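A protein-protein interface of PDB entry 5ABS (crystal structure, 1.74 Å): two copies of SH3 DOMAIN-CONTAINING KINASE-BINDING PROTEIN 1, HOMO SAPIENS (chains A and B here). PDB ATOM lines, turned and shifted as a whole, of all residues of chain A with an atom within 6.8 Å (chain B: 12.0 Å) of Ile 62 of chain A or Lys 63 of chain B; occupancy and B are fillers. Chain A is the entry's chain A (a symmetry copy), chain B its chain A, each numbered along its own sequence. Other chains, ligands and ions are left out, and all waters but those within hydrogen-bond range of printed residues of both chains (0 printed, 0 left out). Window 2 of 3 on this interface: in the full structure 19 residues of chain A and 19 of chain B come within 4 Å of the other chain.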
ATOM      1  N   MET A  57     -33.157   8.743   0.397  1.00  0.00           N
ATOM      2  CA  MET A  57     -34.429   9.248  -0.166  1.00  0.00           C
ATOM      3  C   MET A  57     -34.350  10.718  -0.556  1.00  0.00           C
ATOM      4  O   MET A  57     -34.901  11.118  -1.582  1.00  0.00           O
ATOM      5  CB  MET A  57     -35.568   8.934   0.832  1.00  0.00           C
ATOM      6  CG  MET A  57     -35.983   7.455   0.774  1.00  0.00           C
ATOM      7  SD  MET A  57     -37.399   7.042   2.109  1.00  0.00           S
ATOM      8  CE  MET A  57     -36.552   6.916   3.888  1.00  0.00           C
ATOM      9  N   GLU A  58     -33.651  11.532   0.242  1.00  0.00           N
ATOM     10  CA  GLU A  58     -33.397  12.933  -0.079  1.00  0.00           C
ATOM     11  C   GLU A  58     -32.512  13.134  -1.349  1.00  0.00           C
ATOM     12  O   GLU A  58     -32.838  13.954  -2.218  1.00  0.00           O
ATOM     13  CB  GLU A  58     -32.811  13.685   1.122  1.00  0.00           C
ATOM     14  CG  GLU A  58     -32.826  15.199   1.012  1.00  0.00           C
ATOM     15  CD  GLU A  58     -32.294  15.936   2.242  1.00  0.00           C
ATOM     16  OE1 GLU A  58     -31.828  15.273   3.196  1.00  0.00           O
ATOM     17  OE2 GLU A  58     -32.324  17.200   2.258  1.00  0.00           O
ATOM     18  N   VAL A  59     -31.416  12.380  -1.438  1.00  0.00           N
ATOM     19  CA  VAL A  59     -30.594  12.285  -2.637  1.00  0.00           C
ATOM     20  C   VAL A  59     -31.380  11.813  -3.876  1.00  0.00           C
ATOM     21  O   VAL A  59     -31.291  12.411  -4.939  1.00  0.00           O
ATOM     22  CB  VAL A  59     -29.377  11.404  -2.392  1.00  0.00           C
ATOM     23  CG1 VAL A  59     -28.537  11.128  -3.654  1.00  0.00           C
ATOM     24  CG2 VAL A  59     -28.479  12.100  -1.393  1.00  0.00           C
ATOM     25  N   ASN A  60     -32.166  10.779  -3.733  1.00  0.00           N
ATOM     26  CA  ASN A  60     -33.038  10.369  -4.832  1.00  0.00           C
ATOM     27  C   ASN A  60     -34.049  11.419  -5.285  1.00  0.00           C
ATOM     28  O   ASN A  60     -34.212  11.616  -6.468  1.00  0.00           O
ATOM     29  CB  ASN A  60     -33.679   9.027  -4.507  1.00  0.00           C
ATOM     30  CG  ASN A  60     -32.663   7.890  -4.580  1.00  0.00           C
ATOM     31  OD1 ASN A  60     -31.581   8.007  -5.200  1.00  0.00           O
ATOM     32  ND2 ASN A  60     -32.994   6.785  -3.929  1.00  0.00           N
ATOM     33  N   ASP A  61     -34.653  12.161  -4.360  1.00  0.00           N
ATOM     34  CA  ASP A  61     -35.446  13.319  -4.734  1.00  0.00           C
ATOM     35  C   ASP A  61     -34.675  14.367  -5.520  1.00  0.00           C
ATOM     36  O   ASP A  61     -35.187  14.908  -6.501  1.00  0.00           O
ATOM     37  CB  ASP A  61     -36.045  13.989  -3.516  1.00  0.00           C
ATOM     38  CG  ASP A  61     -37.281  13.282  -3.014  1.00  0.00           C
ATOM     39  OD1 ASP A  61     -37.650  12.190  -3.564  1.00  0.00           O
ATOM     40  OD2 ASP A  61     -37.888  13.848  -2.066  1.00  0.00           O
ATOM     41  N   ILE A  62     -33.445  14.649  -5.103  1.00  0.00           N
ATOM     42  CA  ILE A  62     -32.601  15.592  -5.797  1.00  0.00           C
ATOM     43  C   ILE A  62     -32.346  15.150  -7.231  1.00  0.00           C
ATOM     44  O   ILE A  62     -32.450  15.973  -8.152  1.00  0.00           O
ATOM     45  CB  ILE A  62     -31.256  15.862  -5.057  1.00  0.00           C
ATOM     46  CG1 ILE A  62     -31.496  16.660  -3.761  1.00  0.00           C
ATOM     47  CG2 ILE A  62     -30.293  16.600  -5.959  1.00  0.00           C
ATOM     48  CD1 ILE A  62     -30.239  16.891  -2.917  1.00  0.00           C
ATOM     49  N   LYS A  63     -32.037  13.891  -7.439  1.00  0.00           N
ATOM     50  CA  LYS A  63     -31.855  13.376  -8.799  1.00  0.00           C
ATOM     51  C   LYS A  63     -33.074  13.583  -9.732  1.00  0.00           C
ATOM     52  O   LYS A  63     -32.891  13.838 -10.887  1.00  0.00           O
ATOM     53  CB  LYS A  63     -31.540  11.897  -8.793  1.00  0.00           C
ATOM     54  CG  LYS A  63     -30.176  11.572  -8.228  1.00  0.00           C
ATOM     55  CD  LYS A  63     -29.845  10.088  -8.373  1.00  0.00           C
ATOM     56  CE  LYS A  63     -29.307   9.759  -9.773  1.00  0.00           C
ATOM     57  NZ  LYS A  63     -28.283   8.663  -9.774  1.00  0.00           N
ATOM     58  N   LYS A  64     -34.294  13.444  -9.225  1.00  0.00           N
ATOM     59  CA  LYS A  64     -35.504  13.775  -9.988  1.00  0.00           C
ATOM     60  C   LYS A  64     -35.480  15.206 -10.521  1.00  0.00           C
ATOM     61  O   LYS A  64     -35.865  15.463 -11.648  1.00  0.00           O
ATOM     62  CB  LYS A  64     -36.754  13.595  -9.117  1.00  0.00           C
ATOM     63  N   ALA A  65     -35.045  16.139  -9.686  1.00  0.00           N
ATOM     64  CA  ALA A  65     -35.066  17.563 -10.005  1.00  0.00           C
ATOM     65  C   ALA A  65     -33.947  18.033 -10.912  1.00  0.00           C
ATOM     66  O   ALA A  65     -33.987  19.176 -11.367  1.00  0.00           O
ATOM     67  CB  ALA A  65     -35.018  18.372  -8.725  1.00  0.00           C
ATOM     68  N   LEU A  66     -32.925  17.212 -11.138  1.00  0.00           N
ATOM     69  CA  LEU A  66     -31.902  17.593 -12.109  1.00  0.00           C
ATOM     70  C   LEU A  66     -32.396  17.610 -13.570  1.00  0.00           C
ATOM     71  O   LEU A  66     -31.943  18.526 -14.279  1.00  0.00           O
ATOM     72  CB  LEU A  66     -30.641  16.749 -11.946  1.00  0.00           C
ATOM     73  CG  LEU A  66     -29.884  17.018 -10.642  1.00  0.00           C
ATOM     74  CD1 LEU A  66     -28.395  16.912 -10.903  1.00  0.00           C
ATOM     75  CD2 LEU A  66     -30.186  18.377  -9.992  1.00  0.00           C
ATOM     76  OXT LEU A  66     -33.234  16.807 -14.037  1.00  0.00           O
ATOM     77  N   ARG B  54     -21.330  14.561   7.894  1.00  0.00           N
ATOM     78  CA  ARG B  54     -20.658  15.370   6.902  1.00  0.00           C
ATOM     79  C   ARG B  54     -21.255  15.257   5.484  1.00  0.00           C
ATOM     80  O   ARG B  54     -21.420  16.268   4.763  1.00  0.00           O
ATOM     81  CB  ARG B  54     -19.178  15.002   6.883  1.00  0.00           C
ATOM     82  CG  ARG B  54     -18.353  15.817   5.916  1.00  0.00           C
ATOM     83  CD  ARG B  54     -17.003  16.155   6.538  1.00  0.00           C
ATOM     84  NE  ARG B  54     -16.159  14.963   6.737  1.00  0.00           N
ATOM     85  CZ  ARG B  54     -15.632  14.529   7.896  1.00  0.00           C
ATOM     86  NH1 ARG B  54     -15.842  15.165   9.066  1.00  0.00           N
ATOM     87  NH2 ARG B  54     -14.862  13.436   7.877  1.00  0.00           N
ATOM     88  N   LEU B  55     -21.612  14.040   5.087  1.00  0.00           N
ATOM     89  CA  LEU B  55     -22.323  13.833   3.834  1.00  0.00           C
ATOM     90  C   LEU B  55     -23.661  14.582   3.793  1.00  0.00           C
ATOM     91  O   LEU B  55     -23.970  15.164   2.771  1.00  0.00           O
ATOM     92  CB  LEU B  55     -22.580  12.341   3.577  1.00  0.00           C
ATOM     93  CG  LEU B  55     -23.199  12.006   2.215  1.00  0.00           C
ATOM     94  CD1 LEU B  55     -22.379  12.420   0.997  1.00  0.00           C
ATOM     95  CD2 LEU B  55     -23.318  10.511   2.166  1.00  0.00           C
ATOM     96  N   GLN B  56     -24.438  14.531   4.883  1.00  0.00           N
ATOM     97  CA  GLN B  56     -25.681  15.279   5.022  1.00  0.00           C
ATOM     98  C   GLN B  56     -25.474  16.805   4.808  1.00  0.00           C
ATOM     99  O   GLN B  56     -26.253  17.443   4.122  1.00  0.00           O
ATOM    100  CB  GLN B  56     -26.294  14.981   6.371  1.00  0.00           C
ATOM    101  CG  GLN B  56     -27.725  15.440   6.581  1.00  0.00           C
ATOM    102  CD  GLN B  56     -28.762  14.285   6.699  1.00  0.00           C
ATOM    103  OE1 GLN B  56     -28.570  13.179   7.373  1.00  0.00           O
ATOM    104  NE2 GLN B  56     -29.899  14.536   6.065  1.00  0.00           N
ATOM    105  N   MET B  57     -24.430  17.368   5.417  1.00  0.00           N
ATOM    106  CA  MET B  57     -24.055  18.782   5.198  1.00  0.00           C
ATOM    107  C   MET B  57     -23.696  19.074   3.747  1.00  0.00           C
ATOM    108  O   MET B  57     -24.047  20.131   3.222  1.00  0.00           O
ATOM    109  CB  MET B  57     -22.934  19.155   6.198  1.00  0.00           C
ATOM    110  CG  MET B  57     -23.489  19.387   7.613  1.00  0.00           C
ATOM    111  SD  MET B  57     -22.035  19.797   8.908  1.00  0.00           S
ATOM    112  CE  MET B  57     -21.115  18.109   9.356  1.00  0.00           C
ATOM    113  N   GLU B  58     -23.017  18.136   3.080  1.00  0.00           N
ATOM    114  CA  GLU B  58     -22.717  18.236   1.655  1.00  0.00           C
ATOM    115  C   GLU B  58     -23.984  18.212   0.744  1.00  0.00           C
ATOM    116  O   GLU B  58     -24.117  19.038  -0.170  1.00  0.00           O
ATOM    117  CB  GLU B  58     -21.709  17.166   1.218  1.00  0.00           C
ATOM    118  CG  GLU B  58     -21.074  17.387  -0.143  1.00  0.00           C
ATOM    119  CD  GLU B  58     -20.027  16.343  -0.538  1.00  0.00           C
ATOM    120  OE1 GLU B  58     -19.819  15.371   0.221  1.00  0.00           O
ATOM    121  OE2 GLU B  58     -19.408  16.483  -1.632  1.00  0.00           O
ATOM    122  N   VAL B  59     -24.894  17.275   1.012  1.00  0.00           N
ATOM    123  CA  VAL B  59     -26.219  17.237   0.406  1.00  0.00           C
ATOM    124  C   VAL B  59     -27.035  18.521   0.651  1.00  0.00           C
ATOM    125  O   VAL B  59     -27.604  19.086  -0.273  1.00  0.00           O
ATOM    126  CB  VAL B  59     -26.987  16.004   0.862  1.00  0.00           C
ATOM    127  CG1 VAL B  59     -28.454  15.967   0.388  1.00  0.00           C
ATOM    128  CG2 VAL B  59     -26.299  14.780   0.302  1.00  0.00           C
ATOM    129  N   ASN B  60     -27.062  18.997   1.867  1.00  0.00           N
ATOM    130  CA  ASN B  60     -27.705  20.282   2.133  1.00  0.00           C
ATOM    131  C   ASN B  60     -27.106  21.473   1.390  1.00  0.00           C
ATOM    132  O   ASN B  60     -27.843  22.274   0.859  1.00  0.00           O
ATOM    133  CB  ASN B  60     -27.802  20.507   3.636  1.00  0.00           C
ATOM    134  CG  ASN B  60     -28.843  19.590   4.272  1.00  0.00           C
ATOM    135  OD1 ASN B  60     -29.743  19.040   3.596  1.00  0.00           O
ATOM    136  ND2 ASN B  60     -28.719  19.403   5.577  1.00  0.00           N
ATOM    137  N   ASP B  61     -25.785  21.543   1.260  1.00  0.00           N
ATOM    138  CA  ASP B  61     -25.172  22.520   0.376  1.00  0.00           C
ATOM    139  C   ASP B  61     -25.622  22.410  -1.072  1.00  0.00           C
ATOM    140  O   ASP B  61     -25.888  23.425  -1.718  1.00  0.00           O
ATOM    141  CB  ASP B  61     -23.662  22.419   0.410  1.00  0.00           C
ATOM    142  CG  ASP B  61     -23.062  23.104   1.613  1.00  0.00           C
ATOM    143  OD1 ASP B  61     -23.829  23.605   2.502  1.00  0.00           O
ATOM    144  OD2 ASP B  61     -21.803  23.146   1.647  1.00  0.00           O
ATOM    145  N   ILE B  62     -25.719  21.186  -1.581  1.00  0.00           N
ATOM    146  CA  ILE B  62     -26.181  20.954  -2.929  1.00  0.00           C
ATOM    147  C   ILE B  62     -27.595  21.482  -3.124  1.00  0.00           C
ATOM    148  O   ILE B  62     -27.864  22.152  -4.132  1.00  0.00           O
ATOM    149  CB  ILE B  62     -26.089  19.458  -3.353  1.00  0.00           C
ATOM    150  CG1 ILE B  62     -24.619  19.027  -3.524  1.00  0.00           C
ATOM    151  CG2 ILE B  62     -26.858  19.220  -4.633  1.00  0.00           C
ATOM    152  CD1 ILE B  62     -24.426  17.544  -3.848  1.00  0.00           C
ATOM    153  N   LYS B  63     -28.483  21.216  -2.194  1.00  0.00           N
ATOM    154  CA  LYS B  63     -29.843  21.756  -2.275  1.00  0.00           C
ATOM    155  C   LYS B  63     -29.914  23.300  -2.377  1.00  0.00           C
ATOM    156  O   LYS B  63     -30.756  23.803  -3.062  1.00  0.00           O
ATOM    157  CB  LYS B  63     -30.674  21.347  -1.079  1.00  0.00           C
ATOM    158  CG  LYS B  63     -31.002  19.871  -1.049  1.00  0.00           C
ATOM    159  CD  LYS B  63     -31.957  19.531   0.093  1.00  0.00           C
ATOM    160  CE  LYS B  63     -33.418  19.815  -0.283  1.00  0.00           C
ATOM    161  NZ  LYS B  63     -34.390  18.856   0.340  1.00  0.00           N
ATOM    162  N   LYS B  64     -29.050  24.026  -1.675  1.00  0.00           N
ATOM    163  CA  LYS B  64     -28.938  25.481  -1.830  1.00  0.00           C
ATOM    164  C   LYS B  64     -28.683  25.891  -3.280  1.00  0.00           C
ATOM    165  O   LYS B  64     -29.250  26.852  -3.769  1.00  0.00           O
ATOM    166  CB  LYS B  64     -27.802  26.028  -0.957  1.00  0.00           C
ATOM    167  N   ALA B  65     -27.802  25.165  -3.951  1.00  0.00           N
ATOM    168  CA  ALA B  65     -27.365  25.496  -5.305  1.00  0.00           C
ATOM    169  C   ALA B  65     -28.334  25.105  -6.403  1.00  0.00           C
ATOM    170  O   ALA B  65     -28.127  25.498  -7.550  1.00  0.00           O
ATOM    171  CB  ALA B  65     -26.032  24.835  -5.586  1.00  0.00           C
ATOM    172  N   LEU B  66     -29.348  24.297  -6.099  1.00  0.00           N
ATOM    173  CA  LEU B  66     -30.364  24.014  -7.109  1.00  0.00           C
ATOM    174  C   LEU B  66     -31.249  25.224  -7.469  1.00  0.00           C
ATOM    175  O   LEU B  66     -31.562  25.323  -8.668  1.00  0.00           O
ATOM    176  CB  LEU B  66     -31.198  22.792  -6.729  1.00  0.00           C
ATOM    177  CG  LEU B  66     -30.414  21.478  -6.763  1.00  0.00           C
ATOM    178  CD1 LEU B  66     -31.325  20.370  -7.253  1.00  0.00           C
ATOM    179  CD2 LEU B  66     -29.146  21.507  -7.629  1.00  0.00           C
ATOM    180  OXT LEU B  66     -31.610  26.098  -6.649  1.00  0.00           O
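Met 57 of chain A touches none of the printed residues of chain B.
Glu 58 of chain A touches just these residues of chain B: Gln 56, Asn 60 and Lys 63.
No residue of chain B comes within 4 Å of Asp 61 of chain A.
Of chain B, only Val 59 and Lys 63 come within 4 Å of Ile 62 of chain A.
No residue of chain B comes within 4 Å of Lys 64 of chain A.
No residue of chain B comes within 4 Å of Ala 65 of chain A.
Of chain B, only Leu 66 (3.6 Å) comes within 4 Å of Leu 66 of chain A.
Of the printed residues of chain A, Gln 56 of chain B touches Glu 58.
Of the printed residues of chain A, Val 59 of chain B touches Val 59 (3.8 Å) and Ile 62 (3.9 Å).
Of the printed residues of chain A, Asn 60 of chain B touches Glu 58 (3.4 Å).
Lys 63 of chain B touches just these residues of chain A: Glu 58 and Ile 62.
Of the printed residues of chain A, Leu 66 of chain B touches Leu 66 (3.6 Å).
The nearest residue of chain B that does not touch Ile 62 of chain A is Leu 66 of chain B (4.1 Å).
The nearest residue of chain A that does not touch Lys 63 of chain B is Asp 61 of chain A (6.4 Å).
The nearest printed residue of chain A that does not touch Asn 60 of chain B is Ile 62 of chain A (6.1 Å).
Of the 10 printed residues of chain A, 4 touch a printed residue of chain B.
Printed residues of chain A that touch a printed residue of chain B: Glu 58, Val 59, Ile 62 and Leu 66.
Hydrophobic or aromatic side chains of chain A within 4 Å of the printed part of chain B: Val 59, Ile 62 and Leu 66.
Among the printed residues, 7 pairs touch across the chains.
Among the printed residues, Asp or Glu carboxylates within 4 Å of a Lys or Arg side-chain nitrogen of the other chain: Glu 58 of chain A with Lys 63 of chain B.
Among the printed residues, merely in contact across the chains: Glu 58 of chain A with Gln 56 of chain B, Val 59 of chain A with Val 59 of chain B, Ile 62 of chain A with Val 59 of chain B, Ile 62 of chain A with Lys 63 of chain B and Leu 66 of chain A with Leu 66 of chain B.
Glu 58 of chain A touches Asn 60 of chain B, but with the chains exchanged Asn 60 of chain A does not touch Glu 58 of chain B (11.9 Å).
Glu 58 of chain A touches Lys 63 of chain B, but with the chains exchanged Lys 63 of chain A does not touch Glu 58 of chain B (11.9 Å).
Val 59 of chain A touches its own counterpart, Val 59 of chain B.
Ile 62 of chain A touches Val 59 of chain B, but with the chains exchanged Val 59 of chain A does not touch Ile 62 of chain B (7.2 Å).
Of the 7 pairs that touch across the chains among the printed residues, 2 have their exchanged pair printed and touching as well.
O of Gln 56 of chain B sits close to ND2 of Asn 60 of chain B.
The side-chain amino group of Lys 63 of chain B is in salt-bridge range of the side-chain carboxylate of Glu 58 of chain A (3.3 Å).
The side-chain carboxylate of Glu 58 of chain A lies close to the side-chain amide oxygen of Asn 60 of chain B, 3.4 Å away.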
